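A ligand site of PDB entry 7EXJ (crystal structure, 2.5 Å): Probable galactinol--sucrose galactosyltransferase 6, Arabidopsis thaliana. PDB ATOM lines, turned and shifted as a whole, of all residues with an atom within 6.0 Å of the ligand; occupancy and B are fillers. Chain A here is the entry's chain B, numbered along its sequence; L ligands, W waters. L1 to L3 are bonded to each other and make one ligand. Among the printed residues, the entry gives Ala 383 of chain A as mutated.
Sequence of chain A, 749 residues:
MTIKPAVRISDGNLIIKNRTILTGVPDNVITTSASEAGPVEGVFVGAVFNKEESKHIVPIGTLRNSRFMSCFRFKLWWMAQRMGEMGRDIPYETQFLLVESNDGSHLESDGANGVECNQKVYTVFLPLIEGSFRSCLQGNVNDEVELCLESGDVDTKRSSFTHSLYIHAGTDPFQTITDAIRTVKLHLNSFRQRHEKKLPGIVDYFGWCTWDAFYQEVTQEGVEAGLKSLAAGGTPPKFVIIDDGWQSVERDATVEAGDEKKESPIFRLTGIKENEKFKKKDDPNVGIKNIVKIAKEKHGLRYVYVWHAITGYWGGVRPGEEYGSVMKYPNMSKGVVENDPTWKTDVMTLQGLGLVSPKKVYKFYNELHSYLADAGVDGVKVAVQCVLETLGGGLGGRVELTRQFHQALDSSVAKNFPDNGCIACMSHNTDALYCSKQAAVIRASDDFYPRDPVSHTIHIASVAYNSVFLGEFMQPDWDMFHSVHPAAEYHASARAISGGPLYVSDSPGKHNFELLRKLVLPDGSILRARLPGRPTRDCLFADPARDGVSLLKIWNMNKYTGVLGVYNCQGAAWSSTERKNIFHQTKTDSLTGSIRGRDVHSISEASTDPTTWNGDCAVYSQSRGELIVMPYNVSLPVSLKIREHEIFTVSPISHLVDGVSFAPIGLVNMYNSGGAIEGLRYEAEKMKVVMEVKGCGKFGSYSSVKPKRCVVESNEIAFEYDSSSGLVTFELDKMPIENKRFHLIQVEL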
ATOM      1  N   LYS A  75     -13.501  24.223 -11.002  1.00  0.00           N
ATOM      2  CA  LYS A  75     -12.390  25.037 -11.491  1.00  0.00           C
ATOM      3  C   LYS A  75     -13.011  26.315 -11.968  1.00  0.00           C
ATOM      4  O   LYS A  75     -14.222  26.419 -12.075  1.00  0.00           O
ATOM      5  CB  LYS A  75     -11.671  24.369 -12.682  1.00  0.00           C
ATOM      6  CG  LYS A  75     -10.740  23.232 -12.296  1.00  0.00           C
ATOM      7  CD  LYS A  75     -10.105  22.583 -13.513  1.00  0.00           C
ATOM      8  CE  LYS A  75      -8.963  21.642 -13.139  1.00  0.00           C
ATOM      9  NZ  LYS A  75      -9.106  20.305 -13.774  1.00  0.00           N
ATOM     10  N   TRP A  77     -12.837  27.305 -15.008  1.00  0.00           N
ATOM     11  CA  TRP A  77     -13.243  27.063 -16.362  1.00  0.00           C
ATOM     12  C   TRP A  77     -14.498  26.218 -16.430  1.00  0.00           C
ATOM     13  O   TRP A  77     -15.208  26.265 -17.406  1.00  0.00           O
ATOM     14  CB  TRP A  77     -12.169  26.241 -17.071  1.00  0.00           C
ATOM     15  CG  TRP A  77     -10.787  26.691 -16.832  1.00  0.00           C
ATOM     16  CD1 TRP A  77      -9.759  25.961 -16.329  1.00  0.00           C
ATOM     17  CD2 TRP A  77     -10.276  27.999 -17.047  1.00  0.00           C
ATOM     18  NE1 TRP A  77      -8.634  26.727 -16.245  1.00  0.00           N
ATOM     19  CE2 TRP A  77      -8.923  27.992 -16.686  1.00  0.00           C
ATOM     20  CE3 TRP A  77     -10.824  29.176 -17.561  1.00  0.00           C
ATOM     21  CZ2 TRP A  77      -8.112  29.116 -16.799  1.00  0.00           C
ATOM     22  CZ3 TRP A  77     -10.012  30.294 -17.687  1.00  0.00           C
ATOM     23  CH2 TRP A  77      -8.669  30.257 -17.296  1.00  0.00           C
ATOM     24  N   TRP A  78     -14.712  25.369 -15.434  1.00  0.00           N
ATOM     25  CA  TRP A  78     -15.672  24.280 -15.585  1.00  0.00           C
ATOM     26  C   TRP A  78     -16.527  24.016 -14.349  1.00  0.00           C
ATOM     27  O   TRP A  78     -16.099  24.171 -13.236  1.00  0.00           O
ATOM     28  CB  TRP A  78     -14.955  22.942 -15.917  1.00  0.00           C
ATOM     29  CG  TRP A  78     -14.008  22.958 -16.996  1.00  0.00           C
ATOM     30  CD1 TRP A  78     -12.680  22.819 -16.881  1.00  0.00           C
ATOM     31  CD2 TRP A  78     -14.276  23.185 -18.386  1.00  0.00           C
ATOM     32  NE1 TRP A  78     -12.071  22.914 -18.116  1.00  0.00           N
ATOM     33  CE2 TRP A  78     -13.037  23.143 -19.052  1.00  0.00           C
ATOM     34  CE3 TRP A  78     -15.413  23.369 -19.121  1.00  0.00           C
ATOM     35  CZ2 TRP A  78     -12.931  23.253 -20.398  1.00  0.00           C
ATOM     36  CZ3 TRP A  78     -15.303  23.476 -20.488  1.00  0.00           C
ATOM     37  CH2 TRP A  78     -14.064  23.411 -21.119  1.00  0.00           C
ATOM     38  N   CYS A 209      -9.752  16.219 -33.887  1.00  0.00           N
ATOM     39  CA  CYS A 209      -9.055  17.317 -33.181  1.00  0.00           C
ATOM     40  C   CYS A 209      -7.604  16.934 -32.900  1.00  0.00           C
ATOM     41  O   CYS A 209      -7.340  15.855 -32.435  1.00  0.00           O
ATOM     42  CB  CYS A 209      -9.774  17.654 -31.905  1.00  0.00           C
ATOM     43  SG  CYS A 209      -9.044  19.028 -30.969  1.00  0.00           S
ATOM     44  N   TRP A 211      -5.424  17.923 -30.784  1.00  0.00           N
ATOM     45  CA  TRP A 211      -4.969  18.111 -29.413  1.00  0.00           C
ATOM     46  C   TRP A 211      -4.400  16.876 -28.685  1.00  0.00           C
ATOM     47  O   TRP A 211      -3.292  16.953 -28.163  1.00  0.00           O
ATOM     48  CB  TRP A 211      -6.055  18.787 -28.561  1.00  0.00           C
ATOM     49  CG  TRP A 211      -5.624  18.988 -27.160  1.00  0.00           C
ATOM     50  CD1 TRP A 211      -6.161  18.423 -26.064  1.00  0.00           C
ATOM     51  CD2 TRP A 211      -4.479  19.716 -26.736  1.00  0.00           C
ATOM     52  NE1 TRP A 211      -5.434  18.770 -24.941  1.00  0.00           N
ATOM     53  CE2 TRP A 211      -4.405  19.578 -25.333  1.00  0.00           C
ATOM     54  CE3 TRP A 211      -3.511  20.474 -27.388  1.00  0.00           C
ATOM     55  CZ2 TRP A 211      -3.413  20.228 -24.562  1.00  0.00           C
ATOM     56  CZ3 TRP A 211      -2.537  21.121 -26.633  1.00  0.00           C
ATOM     57  CH2 TRP A 211      -2.483  20.976 -25.237  1.00  0.00           C
ATOM     58  N   TYR A 215      -0.511  17.283 -28.892  1.00  0.00           N
ATOM     59  CA  TYR A 215      -0.505  18.439 -27.983  1.00  0.00           C
ATOM     60  C   TYR A 215       0.126  19.644 -28.689  1.00  0.00           C
ATOM     61  O   TYR A 215      -0.005  19.768 -29.917  1.00  0.00           O
ATOM     62  CB  TYR A 215       0.115  18.059 -26.620  1.00  0.00           C
ATOM     63  CG  TYR A 215      -0.659  16.918 -26.026  1.00  0.00           C
ATOM     64  CD1 TYR A 215      -1.795  17.162 -25.233  1.00  0.00           C
ATOM     65  CD2 TYR A 215      -0.352  15.599 -26.357  1.00  0.00           C
ATOM     66  CE1 TYR A 215      -2.563  16.129 -24.732  1.00  0.00           C
ATOM     67  CE2 TYR A 215      -1.105  14.541 -25.849  1.00  0.00           C
ATOM     68  CZ  TYR A 215      -2.207  14.810 -25.050  1.00  0.00           C
ATOM     69  OH  TYR A 215      -2.940  13.756 -24.590  1.00  0.00           O
ATOM     70  N   GLN A 216       0.810  20.509 -27.956  1.00  0.00           N
ATOM     71  CA  GLN A 216       1.398  21.703 -28.558  1.00  0.00           C
ATOM     72  C   GLN A 216       2.450  21.430 -29.631  1.00  0.00           C
ATOM     73  O   GLN A 216       2.787  22.356 -30.342  1.00  0.00           O
ATOM     74  CB  GLN A 216       1.931  22.627 -27.475  1.00  0.00           C
ATOM     75  CG  GLN A 216       0.840  23.463 -26.830  1.00  0.00           C
ATOM     76  CD  GLN A 216       0.956  23.572 -25.323  1.00  0.00           C
ATOM     77  OE1 GLN A 216       1.372  22.617 -24.681  1.00  0.00           O
ATOM     78  NE2 GLN A 216       0.543  24.729 -24.747  1.00  0.00           N
ATOM     79  N   ASP A 243      -5.569  22.353 -33.035  1.00  0.00           N
ATOM     80  CA  ASP A 243      -5.737  22.810 -31.678  1.00  0.00           C
ATOM     81  C   ASP A 243      -4.527  23.631 -31.293  1.00  0.00           C
ATOM     82  O   ASP A 243      -3.741  23.982 -32.159  1.00  0.00           O
ATOM     83  CB  ASP A 243      -6.044  21.642 -30.747  1.00  0.00           C
ATOM     84  CG  ASP A 243      -7.045  22.028 -29.678  1.00  0.00           C
ATOM     85  OD1 ASP A 243      -8.256  21.681 -29.807  1.00  0.00           O
ATOM     86  OD2 ASP A 243      -6.596  22.723 -28.736  1.00  0.00           O
ATOM     87  N   ASP A 244      -4.422  24.017 -30.021  1.00  0.00           N
ATOM     88  CA  ASP A 244      -3.297  24.822 -29.479  1.00  0.00           C
ATOM     89  C   ASP A 244      -1.986  24.195 -29.965  1.00  0.00           C
ATOM     90  O   ASP A 244      -1.748  22.972 -29.805  1.00  0.00           O
ATOM     91  CB  ASP A 244      -3.388  24.819 -27.963  1.00  0.00           C
ATOM     92  CG  ASP A 244      -2.171  25.352 -27.283  1.00  0.00           C
ATOM     93  OD1 ASP A 244      -1.227  25.813 -27.964  1.00  0.00           O
ATOM     94  OD2 ASP A 244      -2.167  25.258 -26.013  1.00  0.00           O
ATOM     95  N   TRP A 307      -7.733  26.668 -32.929  1.00  0.00           N
ATOM     96  CA  TRP A 307      -7.857  27.072 -31.524  1.00  0.00           C
ATOM     97  C   TRP A 307      -7.244  28.452 -31.255  1.00  0.00           C
ATOM     98  O   TRP A 307      -6.259  28.824 -31.847  1.00  0.00           O
ATOM     99  CB  TRP A 307      -7.126  26.015 -30.685  1.00  0.00           C
ATOM    100  CG  TRP A 307      -7.155  26.110 -29.186  1.00  0.00           C
ATOM    101  CD1 TRP A 307      -7.928  25.398 -28.329  1.00  0.00           C
ATOM    102  CD2 TRP A 307      -6.299  26.903 -28.391  1.00  0.00           C
ATOM    103  NE1 TRP A 307      -7.626  25.709 -27.021  1.00  0.00           N
ATOM    104  CE2 TRP A 307      -6.618  26.641 -27.041  1.00  0.00           C
ATOM    105  CE3 TRP A 307      -5.266  27.800 -28.676  1.00  0.00           C
ATOM    106  CZ2 TRP A 307      -5.966  27.280 -25.969  1.00  0.00           C
ATOM    107  CZ3 TRP A 307      -4.618  28.456 -27.621  1.00  0.00           C
ATOM    108  CH2 TRP A 307      -4.968  28.181 -26.283  1.00  0.00           C
ATOM    109  N   TRP A 314      -2.209  31.755 -23.947  1.00  0.00           N
ATOM    110  CA  TRP A 314      -2.286  31.548 -22.518  1.00  0.00           C
ATOM    111  C   TRP A 314      -1.804  32.736 -21.739  1.00  0.00           C
ATOM    112  O   TRP A 314      -2.410  33.111 -20.747  1.00  0.00           O
ATOM    113  CB  TRP A 314      -1.453  30.354 -22.155  1.00  0.00           C
ATOM    114  CG  TRP A 314      -2.093  29.160 -22.607  1.00  0.00           C
ATOM    115  CD1 TRP A 314      -1.838  28.457 -23.721  1.00  0.00           C
ATOM    116  CD2 TRP A 314      -3.163  28.521 -21.963  1.00  0.00           C
ATOM    117  NE1 TRP A 314      -2.681  27.398 -23.811  1.00  0.00           N
ATOM    118  CE2 TRP A 314      -3.501  27.409 -22.724  1.00  0.00           C
ATOM    119  CE3 TRP A 314      -3.860  28.762 -20.779  1.00  0.00           C
ATOM    120  CZ2 TRP A 314      -4.511  26.557 -22.364  1.00  0.00           C
ATOM    121  CZ3 TRP A 314      -4.860  27.909 -20.417  1.00  0.00           C
ATOM    122  CH2 TRP A 314      -5.187  26.827 -21.208  1.00  0.00           C
ATOM    123  N   LYS A 381     -12.178  27.668 -32.208  1.00  0.00           N
ATOM    124  CA  LYS A 381     -12.492  27.094 -30.940  1.00  0.00           C
ATOM    125  C   LYS A 381     -11.810  28.051 -29.960  1.00  0.00           C
ATOM    126  O   LYS A 381     -10.567  28.087 -29.895  1.00  0.00           O
ATOM    127  CB  LYS A 381     -11.895  25.681 -30.883  1.00  0.00           C
ATOM    128  CG  LYS A 381     -11.801  25.113 -29.477  1.00  0.00           C
ATOM    129  CD  LYS A 381     -11.369  23.654 -29.455  1.00  0.00           C
ATOM    130  CE  LYS A 381     -11.041  23.128 -28.052  1.00  0.00           C
ATOM    131  NZ  LYS A 381     -10.462  21.738 -28.143  1.00  0.00           N
ATOM    132  N   ALA A 383     -10.860  29.223 -26.412  1.00  0.00           N
ATOM    133  CA  ALA A 383     -10.613  28.726 -25.096  1.00  0.00           C
ATOM    134  C   ALA A 383     -10.265  29.853 -24.110  1.00  0.00           C
ATOM    135  O   ALA A 383     -10.218  31.032 -24.495  1.00  0.00           O
ATOM    136  CB  ALA A 383      -9.477  27.747 -25.148  1.00  0.00           C
ATOM    137  N   CYS A 425     -15.135  27.322 -25.209  1.00  0.00           N
ATOM    138  CA  CYS A 425     -14.441  26.360 -24.413  1.00  0.00           C
ATOM    139  C   CYS A 425     -13.890  27.094 -23.161  1.00  0.00           C
ATOM    140  O   CYS A 425     -13.505  28.279 -23.210  1.00  0.00           O
ATOM    141  CB  CYS A 425     -13.394  25.729 -25.292  1.00  0.00           C
ATOM    142  SG  CYS A 425     -12.080  24.914 -24.421  1.00  0.00           S
ATOM    143  N   MET A 426     -13.980  26.416 -22.023  1.00  0.00           N
ATOM    144  CA  MET A 426     -13.551  26.942 -20.752  1.00  0.00           C
ATOM    145  C   MET A 426     -14.363  28.198 -20.374  1.00  0.00           C
ATOM    146  O   MET A 426     -13.810  29.179 -19.928  1.00  0.00           O
ATOM    147  CB  MET A 426     -12.033  27.242 -20.757  1.00  0.00           C
ATOM    148  CG  MET A 426     -11.122  26.030 -21.019  1.00  0.00           C
ATOM    149  SD  MET A 426      -9.432  26.569 -21.378  1.00  0.00           S
ATOM    150  CE  MET A 426      -8.806  26.763 -19.713  1.00  0.00           C
ATOM    151  N   ARG A 443     -18.416  23.589 -25.117  1.00  0.00           N
ATOM    152  CA  ARG A 443     -17.859  22.430 -24.421  1.00  0.00           C
ATOM    153  C   ARG A 443     -18.512  22.363 -23.046  1.00  0.00           C
ATOM    154  O   ARG A 443     -18.544  23.393 -22.309  1.00  0.00           O
ATOM    155  CB  ARG A 443     -16.359  22.583 -24.306  1.00  0.00           C
ATOM    156  CG  ARG A 443     -15.589  22.216 -25.546  1.00  0.00           C
ATOM    157  CD  ARG A 443     -15.361  20.737 -25.561  1.00  0.00           C
ATOM    158  NE  ARG A 443     -14.794  20.372 -24.282  1.00  0.00           N
ATOM    159  CZ  ARG A 443     -13.518  20.481 -23.956  1.00  0.00           C
ATOM    160  NH1 ARG A 443     -12.614  20.884 -24.851  1.00  0.00           N
ATOM    161  NH2 ARG A 443     -13.159  20.167 -22.735  1.00  0.00           N
ATOM    162  N   SER A 445     -17.770  20.288 -20.442  1.00  0.00           N
ATOM    163  CA  SER A 445     -16.977  19.886 -19.303  1.00  0.00           C
ATOM    164  C   SER A 445     -15.496  20.102 -19.508  1.00  0.00           C
ATOM    165  O   SER A 445     -15.026  20.386 -20.606  1.00  0.00           O
ATOM    166  CB  SER A 445     -17.171  18.392 -19.071  1.00  0.00           C
ATOM    167  OG  SER A 445     -16.512  17.711 -20.120  1.00  0.00           O
ATOM    168  N   ASP A 446     -14.775  19.947 -18.413  1.00  0.00           N
ATOM    169  CA  ASP A 446     -13.368  19.650 -18.418  1.00  0.00           C
ATOM    170  C   ASP A 446     -13.043  18.579 -19.475  1.00  0.00           C
ATOM    171  O   ASP A 446     -13.912  17.825 -19.903  1.00  0.00           O
ATOM    172  CB  ASP A 446     -12.953  19.139 -17.020  1.00  0.00           C
ATOM    173  CG  ASP A 446     -11.494  19.396 -16.708  1.00  0.00           C
ATOM    174  OD1 ASP A 446     -10.794  20.010 -17.540  1.00  0.00           O
ATOM    175  OD2 ASP A 446     -11.066  18.981 -15.611  1.00  0.00           O
ATOM    176  N   ASP A 447     -11.752  18.558 -19.861  1.00  0.00           N
ATOM    177  CA  ASP A 447     -11.249  17.868 -21.017  1.00  0.00           C
ATOM    178  C   ASP A 447     -11.372  16.382 -20.829  1.00  0.00           C
ATOM    179  O   ASP A 447     -11.337  15.877 -19.699  1.00  0.00           O
ATOM    180  CB  ASP A 447      -9.734  18.095 -21.231  1.00  0.00           C
ATOM    181  CG  ASP A 447      -9.299  19.554 -21.403  1.00  0.00           C
ATOM    182  OD1 ASP A 447     -10.081  20.541 -21.411  1.00  0.00           O
ATOM    183  OD2 ASP A 447      -8.068  19.716 -21.537  1.00  0.00           O
ATOM    184  N   TYR A 449      -9.420  13.180 -20.736  1.00  0.00           N
ATOM    185  CA  TYR A 449      -8.038  12.892 -20.343  1.00  0.00           C
ATOM    186  C   TYR A 449      -7.735  11.408 -20.633  1.00  0.00           C
ATOM    187  O   TYR A 449      -8.114  10.541 -19.869  1.00  0.00           O
ATOM    188  CB  TYR A 449      -7.848  13.162 -18.860  1.00  0.00           C
ATOM    189  CG  TYR A 449      -7.970  14.604 -18.474  1.00  0.00           C
ATOM    190  CD1 TYR A 449      -7.045  15.511 -18.935  1.00  0.00           C
ATOM    191  CD2 TYR A 449      -8.990  15.051 -17.627  1.00  0.00           C
ATOM    192  CE1 TYR A 449      -7.122  16.851 -18.603  1.00  0.00           C
ATOM    193  CE2 TYR A 449      -9.074  16.372 -17.272  1.00  0.00           C
ATOM    194  CZ  TYR A 449      -8.130  17.290 -17.767  1.00  0.00           C
ATOM    195  OH  TYR A 449      -8.168  18.637 -17.467  1.00  0.00           O
ATOM    196  N   ARG A 451      -5.166   9.701 -20.296  1.00  0.00           N
ATOM    197  CA  ARG A 451      -4.219   9.008 -19.400  1.00  0.00           C
ATOM    198  C   ARG A 451      -4.649   8.944 -17.946  1.00  0.00           C
ATOM    199  O   ARG A 451      -3.972   8.280 -17.174  1.00  0.00           O
ATOM    200  CB  ARG A 451      -2.809   9.597 -19.552  1.00  0.00           C
ATOM    201  CG  ARG A 451      -2.322   9.532 -20.990  1.00  0.00           C
ATOM    202  CD  ARG A 451      -0.914  10.076 -21.169  1.00  0.00           C
ATOM    203  NE  ARG A 451      -0.779  11.440 -20.635  1.00  0.00           N
ATOM    204  CZ  ARG A 451      -1.161  12.571 -21.242  1.00  0.00           C
ATOM    205  NH1 ARG A 451      -1.727  12.543 -22.435  1.00  0.00           N
ATOM    206  NH2 ARG A 451      -0.948  13.740 -20.635  1.00  0.00           N
ATOM    207  N   ASP A 479     -16.912  16.965 -26.162  1.00  0.00           N
ATOM    208  CA  ASP A 479     -15.464  16.954 -26.288  1.00  0.00           C
ATOM    209  C   ASP A 479     -14.965  15.717 -27.053  1.00  0.00           C
ATOM    210  O   ASP A 479     -15.695  14.770 -27.305  1.00  0.00           O
ATOM    211  CB  ASP A 479     -14.762  17.082 -24.908  1.00  0.00           C
ATOM    212  CG  ASP A 479     -13.299  17.472 -25.027  1.00  0.00           C
ATOM    213  OD1 ASP A 479     -12.908  18.040 -26.061  1.00  0.00           O
ATOM    214  OD2 ASP A 479     -12.529  17.179 -24.096  1.00  0.00           O
ATOM    215  N   MET A 480     -13.731  15.779 -27.502  1.00  0.00           N
ATOM    216  CA  MET A 480     -13.070  14.662 -28.197  1.00  0.00           C
ATOM    217  C   MET A 480     -12.914  13.391 -27.347  1.00  0.00           C
ATOM    218  O   MET A 480     -13.191  13.383 -26.151  1.00  0.00           O
ATOM    219  CB  MET A 480     -11.690  15.142 -28.664  1.00  0.00           C
ATOM    220  CG  MET A 480     -10.746  15.504 -27.524  1.00  0.00           C
ATOM    221  SD  MET A 480      -9.402  16.603 -28.011  1.00  0.00           S
ATOM    222  CE  MET A 480     -10.114  18.222 -27.779  1.00  0.00           C
HETATM  223  C1  LIG L   1      -3.232  21.549 -16.853  1.00  0.00           C
HETATM  224  C2  LIG L   1      -3.796  21.308 -18.139  1.00  0.00           C
HETATM  225  C3  LIG L   1      -3.585  19.772 -18.643  1.00  0.00           C
HETATM  226  C4  LIG L   1      -3.197  19.807 -19.856  1.00  0.00           C
HETATM  227  C5  LIG L   1      -3.041  21.419 -20.318  1.00  0.00           C
HETATM  228  C6  LIG L   1      -3.994  21.884 -21.379  1.00  0.00           C
HETATM  229  O1  LIG L   1      -1.865  21.500 -16.915  1.00  0.00           O
HETATM  230  O2  LIG L   1      -5.238  21.516 -18.086  1.00  0.00           O
HETATM  231  O3  LIG L   1      -4.774  18.907 -18.375  1.00  0.00           O
HETATM  232  O4  LIG L   1      -3.867  18.876 -20.824  1.00  0.00           O
HETATM  233  O5  LIG L   1      -3.151  22.166 -19.218  1.00  0.00           O
HETATM  234  O6  LIG L   1      -3.484  23.009 -22.066  1.00  0.00           O
HETATM  235  C1  LG2 L   2      -5.626  22.902 -17.915  1.00  0.00           C
HETATM  236  C2  LG2 L   2      -6.836  22.892 -17.020  1.00  0.00           C
HETATM  237  C3  LG2 L   2      -7.956  22.343 -17.681  1.00  0.00           C
HETATM  238  C4  LG2 L   2      -8.348  23.115 -18.920  1.00  0.00           C
HETATM  239  C5  LG2 L   2      -7.184  23.520 -19.923  1.00  0.00           C
HETATM  240  C6  LG2 L   2      -7.260  22.875 -21.253  1.00  0.00           C
HETATM  241  O1  LG2 L   2      -6.581  22.110 -15.776  1.00  0.00           O
HETATM  242  O2  LG2 L   2      -9.076  22.308 -16.685  1.00  0.00           O
HETATM  243  O3  LG2 L   2      -9.405  22.444 -19.585  1.00  0.00           O
HETATM  244  O4  LG2 L   2      -5.793  23.436 -19.296  1.00  0.00           O
HETATM  245  O5  LG2 L   2      -8.283  23.606 -21.938  1.00  0.00           O
HETATM  246  C1  LG3 L   3      -8.381  23.663 -23.288  1.00  0.00           C
HETATM  247  C2  LG3 L   3      -9.050  22.396 -23.707  1.00  0.00           C
HETATM  248  C3  LG3 L   3      -8.870  22.043 -25.092  1.00  0.00           C
HETATM  249  C4  LG3 L   3      -7.591  22.544 -25.707  1.00  0.00           C
HETATM  250  C5  LG3 L   3      -6.505  22.810 -24.694  1.00  0.00           C
HETATM  251  C6  LG3 L   3      -5.249  23.331 -25.331  1.00  0.00           C
HETATM  252  O1  LG3 L   3     -10.482  22.576 -23.520  1.00  0.00           O
HETATM  253  O2  LG3 L   3      -8.959  20.585 -25.049  1.00  0.00           O
HETATM  254  O3  LG3 L   3      -7.143  21.577 -26.612  1.00  0.00           O
HETATM  255  O4  LG3 L   3      -7.032  23.879 -23.873  1.00  0.00           O
HETATM  256  O5  LG3 L   3      -4.329  23.905 -24.419  1.00  0.00           O
HETATM  257  O   HOH W   1      -6.069  17.964 -22.020  1.00  0.00           O
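The side-chain carboxylate (OD2) of Asp 243 lies within hydrogen-bond range of an oxygen (O3) of LG3 L3, at 2.5 Å. The side-chain carboxylate of Asp 447 lies within hydrogen-bond range of an oxygen (O3) of LG2 L2, 2.7 Å away. The side-chain sulfur (SG) of Cys 425 sits at hydrogen-bond distance from an oxygen (O1) of LG3 L3, at 3.0 Å. The side-chain carboxylate of Asp 446 sits at hydrogen-bond distance from an oxygen (O2) of LG2 L2 (3.0 Å). An oxygen (O5) of LG3 L3 sits at hydrogen-bond distance from the side-chain carboxylate (OD2) of Asp 244 (3.0 Å). An oxygen (O1) of LG3 L3 lies within hydrogen-bond range of the guanidinium group (NH1) of Arg 443, at 3.0 Å. An oxygen (O3) of LG2 L2 lies within hydrogen-bond range of the indole nitrogen (NE1) of Trp 78, at 3.1 Å.
OD1 of Asp 243 is in hydrogen-bond range of SG of Cys 209 (3.0 Å). The side-chain carboxylate (OD1) of Asp 447 is in salt-bridge range of the guanidinium group (NH2) of Arg 443, 3.4 Å away. The side-chain carboxylate (OD1) of Asp 446 is in hydrogen-bond range of the side-chain hydroxyl (OH) of Tyr 449 (3.0 Å). The side-chain amino group of Lys 75 lies within salt-bridge range of the side-chain carboxylate of Asp 446 (3.0 Å). The indole nitrogen (NE1) of Trp 314 sits at hydrogen-bond distance from the side-chain carboxylate (OD2) of Asp 244 (3.1 Å). The side-chain amide nitrogen of Gln 216 sits at hydrogen-bond distance from the side-chain carboxylate of Asp 244, 3.0 Å away. The guanidinium group (NH2) of Arg 443 lies within hydrogen-bond range of the backbone carbonyl oxygen (O) of Ser 445 (2.8 Å). The backbone NH (N) of Trp 211 lies close to the side-chain sulfur (SG) of Cys 209, 3.8 Å away.
The side-chain sulfur (SD) of Met 426 sits close to an oxygen (O5) of LG2 L2 (3.2 Å). CD of Lys 75 touches O2 of LG2 L2, at 3.3 Å. CD1 of Trp 77 touches O2 of LG2 L2 (3.7 Å). Trp 211 touches the ligand. Trp 307 touches the ligand. CZ2 of Trp 314 touches O5 of LG3 L3 (3.4 Å). NZ of Lys 381 touches C3 of LG3 L3 (3.5 Å). CE1 of Tyr 449 touches O3 of LIG L1 (3.1 Å). CE of Met 480 touches O2 of LG3 L3, at 3.8 Å. Hydrophobic or aromatic side chains that line the ligand: Trp 77, Trp 78, Trp 211, Trp 307, Trp 314, Met 426, Tyr 449 and Met 480. The nearest printed residue that does not touch the ligand is Ala 383 (4.6 Å).
Water W1 lies within hydrogen-bond range of O4 of LIG L1 (2.7 Å), OD2 of Asp 447 (2.7 Å) and NE1 of Trp 211 (3.1 Å).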
